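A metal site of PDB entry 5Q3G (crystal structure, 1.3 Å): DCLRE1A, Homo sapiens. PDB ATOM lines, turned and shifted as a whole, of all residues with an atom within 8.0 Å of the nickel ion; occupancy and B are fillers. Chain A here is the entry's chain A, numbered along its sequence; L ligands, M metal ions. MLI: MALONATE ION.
The side-chain hydroxyl (OG1) of Thr 34 is in hydrogen-bond range of a ring nitrogen (ND1) of His 35 (2.9 Å). A ring nitrogen (NE2) of His 37 sits at hydrogen-bond distance from the backbone carbonyl oxygen (O) of Ile 184 (2.9 Å). ND1 of His 96 lies within hydrogen-bond range of O of Glu 296 (2.8 Å). NE2 of His 40 sits close to OD2 of Asp 118 (3.4 Å).
The nickel ion is bound by O8 of the ligand (2.1 Å), O7 of the ligand (2.1 Å), OD2 of Asp 118 (2.2 Å), NE2 of His 35 (2.2 Å), ND1 of His 37 (2.2 Å) and NE2 of His 96 (2.2 Å).
Of the 20 residues printed, 4 come within 4 Å of the nickel ion.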
ATOM      1  N   ASP A  18     -14.463  -8.372  11.803  1.00  0.00           N
ATOM      2  CA  ASP A  18     -15.415  -9.435  12.275  1.00  0.00           C
ATOM      3  C   ASP A  18     -16.916  -8.967  12.180  1.00  0.00           C
ATOM      4  O   ASP A  18     -17.724  -9.282  13.067  1.00  0.00           O
ATOM      5  CB  ASP A  18     -14.993 -10.002  13.605  1.00  0.00           C
ATOM      6  CG  ASP A  18     -13.550 -10.611  13.600  1.00  0.00           C
ATOM      7  OD1 ASP A  18     -13.000 -10.810  12.529  1.00  0.00           O
ATOM      8  OD2 ASP A  18     -13.141 -10.891  14.773  1.00  0.00           O
ATOM      9  N   THR A  34     -10.503 -11.819  11.753  1.00  0.00           N
ATOM     10  CA  THR A  34      -9.369 -12.178  12.641  1.00  0.00           C
ATOM     11  C   THR A  34      -9.091 -13.695  12.670  1.00  0.00           C
ATOM     12  O   THR A  34      -7.948 -14.117  12.815  1.00  0.00           O
ATOM     13  CB  THR A  34      -9.545 -11.642  14.072  1.00  0.00           C
ATOM     14  OG1 THR A  34     -10.733 -12.264  14.694  1.00  0.00           O
ATOM     15  CG2 THR A  34      -9.620 -10.133  14.103  1.00  0.00           C
ATOM     16  N   HIS A  35     -10.130 -14.520  12.581  1.00  0.00           N
ATOM     17  CA  HIS A  35     -10.044 -15.978  12.731  1.00  0.00           C
ATOM     18  C   HIS A  35     -11.320 -16.675  12.295  1.00  0.00           C
ATOM     19  O   HIS A  35     -12.419 -16.048  12.353  1.00  0.00           O
ATOM     20  CB  HIS A  35      -9.534 -16.398  14.165  1.00  0.00           C
ATOM     21  CG  HIS A  35     -10.503 -16.200  15.266  1.00  0.00           C
ATOM     22  ND1 HIS A  35     -10.938 -14.971  15.765  1.00  0.00           N
ATOM     23  CD2 HIS A  35     -11.096 -17.115  16.064  1.00  0.00           C
ATOM     24  CE1 HIS A  35     -11.747 -15.191  16.821  1.00  0.00           C
ATOM     25  NE2 HIS A  35     -11.827 -16.464  17.006  1.00  0.00           N
ATOM     26  N   PHE A  36     -11.145 -17.957  12.019  1.00  0.00           N
ATOM     27  CA  PHE A  36     -12.293 -18.833  11.585  1.00  0.00           C
ATOM     28  C   PHE A  36     -13.053 -19.472  12.737  1.00  0.00           C
ATOM     29  O   PHE A  36     -13.046 -20.772  12.873  1.00  0.00           O
ATOM     30  CB  PHE A  36     -11.763 -19.873  10.569  1.00  0.00           C
ATOM     31  CG  PHE A  36     -12.860 -20.545   9.728  1.00  0.00           C
ATOM     32  CD1 PHE A  36     -13.447 -19.851   8.657  1.00  0.00           C
ATOM     33  CD2 PHE A  36     -13.278 -21.851   9.964  1.00  0.00           C
ATOM     34  CE1 PHE A  36     -14.461 -20.471   7.858  1.00  0.00           C
ATOM     35  CE2 PHE A  36     -14.280 -22.473   9.192  1.00  0.00           C
ATOM     36  CZ  PHE A  36     -14.817 -21.816   8.138  1.00  0.00           C
ATOM     37  N   HIS A  37     -13.707 -18.666  13.566  1.00  0.00           N
ATOM     38  CA  HIS A  37     -14.682 -19.134  14.571  1.00  0.00           C
ATOM     39  C   HIS A  37     -16.076 -18.506  14.169  1.00  0.00           C
ATOM     40  O   HIS A  37     -16.188 -17.315  13.790  1.00  0.00           O
ATOM     41  CB  HIS A  37     -14.339 -18.765  16.019  1.00  0.00           C
ATOM     42  CG  HIS A  37     -13.328 -19.693  16.654  1.00  0.00           C
ATOM     43  ND1 HIS A  37     -12.582 -19.374  17.787  1.00  0.00           N
ATOM     44  CD2 HIS A  37     -12.964 -20.947  16.328  1.00  0.00           C
ATOM     45  CE1 HIS A  37     -11.837 -20.406  18.145  1.00  0.00           C
ATOM     46  NE2 HIS A  37     -12.060 -21.354  17.260  1.00  0.00           N
ATOM     47  N   SER A  38     -17.143 -19.332  14.324  1.00  0.00           N
ATOM     48  CA  SER A  38     -18.480 -19.013  13.763  1.00  0.00           C
ATOM     49  C   SER A  38     -19.043 -17.675  14.255  1.00  0.00           C
ATOM     50  O   SER A  38     -19.620 -16.980  13.382  1.00  0.00           O
ATOM     51  CB  SER A  38     -19.393 -20.238  13.895  1.00  0.00           C
ATOM     52  OG  SER A  38     -19.687 -20.508  15.226  1.00  0.00           O
ATOM     53  N   ASP A  39     -18.900 -17.297  15.523  1.00  0.00           N
ATOM     54  CA  ASP A  39     -19.435 -15.986  15.997  1.00  0.00           C
ATOM     55  C   ASP A  39     -18.786 -14.820  15.242  1.00  0.00           C
ATOM     56  O   ASP A  39     -19.375 -13.689  15.146  1.00  0.00           O
ATOM     57  CB  ASP A  39     -19.262 -15.802  17.498  1.00  0.00           C
ATOM     58  CG  ASP A  39     -20.318 -16.530  18.376  1.00  0.00           C
ATOM     59  OD1 ASP A  39     -21.231 -17.151  17.770  1.00  0.00           O
ATOM     60  OD2 ASP A  39     -20.142 -16.482  19.598  1.00  0.00           O
ATOM     61  N   HIS A  40     -17.544 -15.000  14.732  1.00  0.00           N
ATOM     62  CA  HIS A  40     -16.763 -13.948  14.054  1.00  0.00           C
ATOM     63  C   HIS A  40     -16.972 -13.949  12.582  1.00  0.00           C
ATOM     64  O   HIS A  40     -17.057 -12.828  11.969  1.00  0.00           O
ATOM     65  CB  HIS A  40     -15.233 -14.109  14.424  1.00  0.00           C
ATOM     66  CG  HIS A  40     -14.993 -13.936  15.865  1.00  0.00           C
ATOM     67  ND1 HIS A  40     -14.464 -12.781  16.443  1.00  0.00           N
ATOM     68  CD2 HIS A  40     -15.211 -14.777  16.918  1.00  0.00           C
ATOM     69  CE1 HIS A  40     -14.437 -12.913  17.738  1.00  0.00           C
ATOM     70  NE2 HIS A  40     -14.899 -14.109  18.055  1.00  0.00           N
ATOM     71  N   HIS A  96      -4.202 -17.999  19.574  1.00  0.00           N
ATOM     72  CA  HIS A  96      -5.611 -18.460  19.765  1.00  0.00           C
ATOM     73  C   HIS A  96      -5.701 -19.754  19.012  1.00  0.00           C
ATOM     74  O   HIS A  96      -5.032 -20.732  19.448  1.00  0.00           O
ATOM     75  CB  HIS A  96      -6.578 -17.342  19.347  1.00  0.00           C
ATOM     76  CG  HIS A  96      -8.063 -17.591  19.556  1.00  0.00           C
ATOM     77  ND1 HIS A  96      -8.586 -18.024  20.753  1.00  0.00           N
ATOM     78  CD2 HIS A  96      -9.090 -17.560  18.682  1.00  0.00           C
ATOM     79  CE1 HIS A  96      -9.919 -18.186  20.598  1.00  0.00           C
ATOM     80  NE2 HIS A  96     -10.260 -17.883  19.374  1.00  0.00           N
ATOM     81  N   CYS A  97      -6.499 -19.909  17.992  1.00  0.00           N
ATOM     82  CA  CYS A  97      -6.575 -21.124  17.117  1.00  0.00           C
ATOM     83  C   CYS A  97      -5.697 -20.956  15.876  1.00  0.00           C
ATOM     84  O   CYS A  97      -5.214 -19.841  15.602  1.00  0.00           O
ATOM     85  CB  CYS A  97      -8.069 -21.341  16.768  1.00  0.00           C
ATOM     86  SG  CYS A  97      -8.805 -20.015  15.742  1.00  0.00           S
ATOM     87  N   ALA A 100      -5.377 -17.500  13.559  1.00  0.00           N
ATOM     88  CA  ALA A 100      -5.911 -16.341  14.285  1.00  0.00           C
ATOM     89  C   ALA A 100      -4.828 -15.255  14.368  1.00  0.00           C
ATOM     90  O   ALA A 100      -3.672 -15.514  14.715  1.00  0.00           O
ATOM     91  CB  ALA A 100      -6.395 -16.737  15.646  1.00  0.00           C
ATOM     92  N   GLY A 117      -8.358  -9.259  18.157  1.00  0.00           N
ATOM     93  CA  GLY A 117      -9.281 -10.371  17.887  1.00  0.00           C
ATOM     94  C   GLY A 117      -9.477 -11.155  19.141  1.00  0.00           C
ATOM     95  O   GLY A 117      -9.591 -10.595  20.216  1.00  0.00           O
ATOM     96  N   ASP A 118      -9.586 -12.489  18.983  1.00  0.00           N
ATOM     97  CA  ASP A 118      -9.457 -13.395  20.163  1.00  0.00           C
ATOM     98  C   ASP A 118      -7.968 -13.766  20.400  1.00  0.00           C
ATOM     99  O   ASP A 118      -7.275 -14.065  19.405  1.00  0.00           O
ATOM    100  CB  ASP A 118     -10.297 -14.678  19.996  1.00  0.00           C
ATOM    101  CG  ASP A 118     -11.796 -14.543  20.205  1.00  0.00           C
ATOM    102  OD1 ASP A 118     -12.245 -13.484  20.693  1.00  0.00           O
ATOM    103  OD2 ASP A 118     -12.467 -15.563  19.956  1.00  0.00           O
ATOM    104  N   PHE A 119      -7.512 -13.723  21.621  1.00  0.00           N
ATOM    105  CA  PHE A 119      -6.079 -14.004  21.902  1.00  0.00           C
ATOM    106  C   PHE A 119      -5.856 -14.619  23.260  1.00  0.00           C
ATOM    107  O   PHE A 119      -6.686 -14.445  24.161  1.00  0.00           O
ATOM    108  CB  PHE A 119      -5.151 -12.743  21.658  1.00  0.00           C
ATOM    109  CG  PHE A 119      -4.964 -11.748  22.796  1.00  0.00           C
ATOM    110  CD1 PHE A 119      -3.749 -11.159  23.065  1.00  0.00           C
ATOM    111  CD2 PHE A 119      -6.036 -11.287  23.608  1.00  0.00           C
ATOM    112  CE1 PHE A 119      -3.572 -10.222  24.043  1.00  0.00           C
ATOM    113  CE2 PHE A 119      -5.866 -10.354  24.644  1.00  0.00           C
ATOM    114  CZ  PHE A 119      -4.615  -9.810  24.829  1.00  0.00           C
ATOM    115  N   ASP A 141      -9.865  -8.466  23.664  1.00  0.00           N
ATOM    116  CA  ASP A 141     -10.586  -9.717  24.020  1.00  0.00           C
ATOM    117  C   ASP A 141     -10.588  -9.835  25.530  1.00  0.00           C
ATOM    118  O   ASP A 141      -9.608 -10.231  26.169  1.00  0.00           O
ATOM    119  CB  ASP A 141      -9.877 -10.944  23.407  1.00  0.00           C
ATOM    120  CG  ASP A 141     -10.411 -12.281  23.931  1.00  0.00           C
ATOM    121  OD1 ASP A 141     -11.478 -12.291  24.583  1.00  0.00           O
ATOM    122  OD2 ASP A 141      -9.720 -13.296  23.654  1.00  0.00           O
ATOM    123  N   THR A 143     -12.756 -11.809  27.316  1.00  0.00           N
ATOM    124  CA  THR A 143     -13.516 -12.998  27.699  1.00  0.00           C
ATOM    125  C   THR A 143     -13.414 -13.332  29.140  1.00  0.00           C
ATOM    126  O   THR A 143     -14.492 -13.522  29.829  1.00  0.00           O
ATOM    127  CB  THR A 143     -13.060 -14.231  26.844  1.00  0.00           C
ATOM    128  OG1 THR A 143     -13.321 -14.031  25.452  1.00  0.00           O
ATOM    129  CG2 THR A 143     -13.789 -15.492  27.249  1.00  0.00           C
ATOM    130  N   SER A 183     -15.115 -26.945  16.626  1.00  0.00           N
ATOM    131  CA  SER A 183     -14.533 -25.810  15.943  1.00  0.00           C
ATOM    132  C   SER A 183     -13.044 -26.104  15.781  1.00  0.00           C
ATOM    133  O   SER A 183     -12.533 -27.051  16.426  1.00  0.00           O
ATOM    134  CB  SER A 183     -14.650 -24.487  16.737  1.00  0.00           C
ATOM    135  OG  SER A 183     -14.052 -24.616  18.031  1.00  0.00           O
ATOM    136  N   ILE A 184     -12.321 -25.336  15.023  1.00  0.00           N
ATOM    137  CA  ILE A 184     -10.859 -25.386  15.035  1.00  0.00           C
ATOM    138  C   ILE A 184     -10.339 -24.849  16.366  1.00  0.00           C
ATOM    139  O   ILE A 184     -11.119 -24.106  17.111  1.00  0.00           O
ATOM    140  CB  ILE A 184     -10.219 -24.615  13.856  1.00  0.00           C
ATOM    141  CG1 ILE A 184     -10.434 -23.132  13.892  1.00  0.00           C
ATOM    142  CG2 ILE A 184     -10.641 -25.238  12.514  1.00  0.00           C
ATOM    143  CD1 ILE A 184      -9.594 -22.386  12.907  1.00  0.00           C
ATOM    144  N   GLU A 296      -7.754 -21.266  25.090  1.00  0.00           N
ATOM    145  CA  GLU A 296      -7.147 -20.424  24.024  1.00  0.00           C
ATOM    146  C   GLU A 296      -7.476 -18.890  24.169  1.00  0.00           C
ATOM    147  O   GLU A 296      -7.354 -18.090  23.225  1.00  0.00           O
ATOM    148  CB  GLU A 296      -7.411 -20.946  22.610  1.00  0.00           C
ATOM    149  CG  GLU A 296      -6.684 -22.318  22.363  1.00  0.00           C
ATOM    150  CD  GLU A 296      -6.758 -22.880  20.958  1.00  0.00           C
ATOM    151  OE1 GLU A 296      -7.685 -22.511  20.180  1.00  0.00           O
ATOM    152  OE2 GLU A 296      -5.856 -23.770  20.664  1.00  0.00           O
ATOM    153  N   HIS A 297      -7.916 -18.525  25.382  1.00  0.00           N
ATOM    154  CA  HIS A 297      -8.044 -17.110  25.764  1.00  0.00           C
ATOM    155  C   HIS A 297      -7.182 -16.771  26.991  1.00  0.00           C
ATOM    156  O   HIS A 297      -6.880 -17.643  27.838  1.00  0.00           O
ATOM    157  CB  HIS A 297      -9.541 -16.723  26.124  1.00  0.00           C
ATOM    158  CG  HIS A 297     -10.504 -16.855  25.016  1.00  0.00           C
ATOM    159  ND1 HIS A 297     -10.778 -15.865  24.091  1.00  0.00           N
ATOM    160  CD2 HIS A 297     -11.397 -17.881  24.721  1.00  0.00           C
ATOM    161  CE1 HIS A 297     -11.740 -16.272  23.275  1.00  0.00           C
ATOM    162  NE2 HIS A 297     -12.090 -17.488  23.628  1.00  0.00           N
HETATM  163  C1  MLI L   1     -15.077 -18.907  20.243  1.00  0.00           C
HETATM  164  C2  MLI L   1     -13.960 -18.770  21.244  1.00  0.00           C
HETATM  165  C3  MLI L   1     -15.331 -17.627  19.437  1.00  0.00           C
HETATM  166  O6  MLI L   1     -14.013 -19.075  22.404  1.00  0.00           O
HETATM  167  O7  MLI L   1     -12.878 -18.403  20.759  1.00  0.00           O
HETATM  168  O8  MLI L   1     -14.408 -17.123  18.749  1.00  0.00           O
HETATM  169  O9  MLI L   1     -16.554 -17.181  19.276  1.00  0.00           O
HETATM  170 NI    NI M   1     -12.383 -17.469  18.889  1.00  0.00          NI
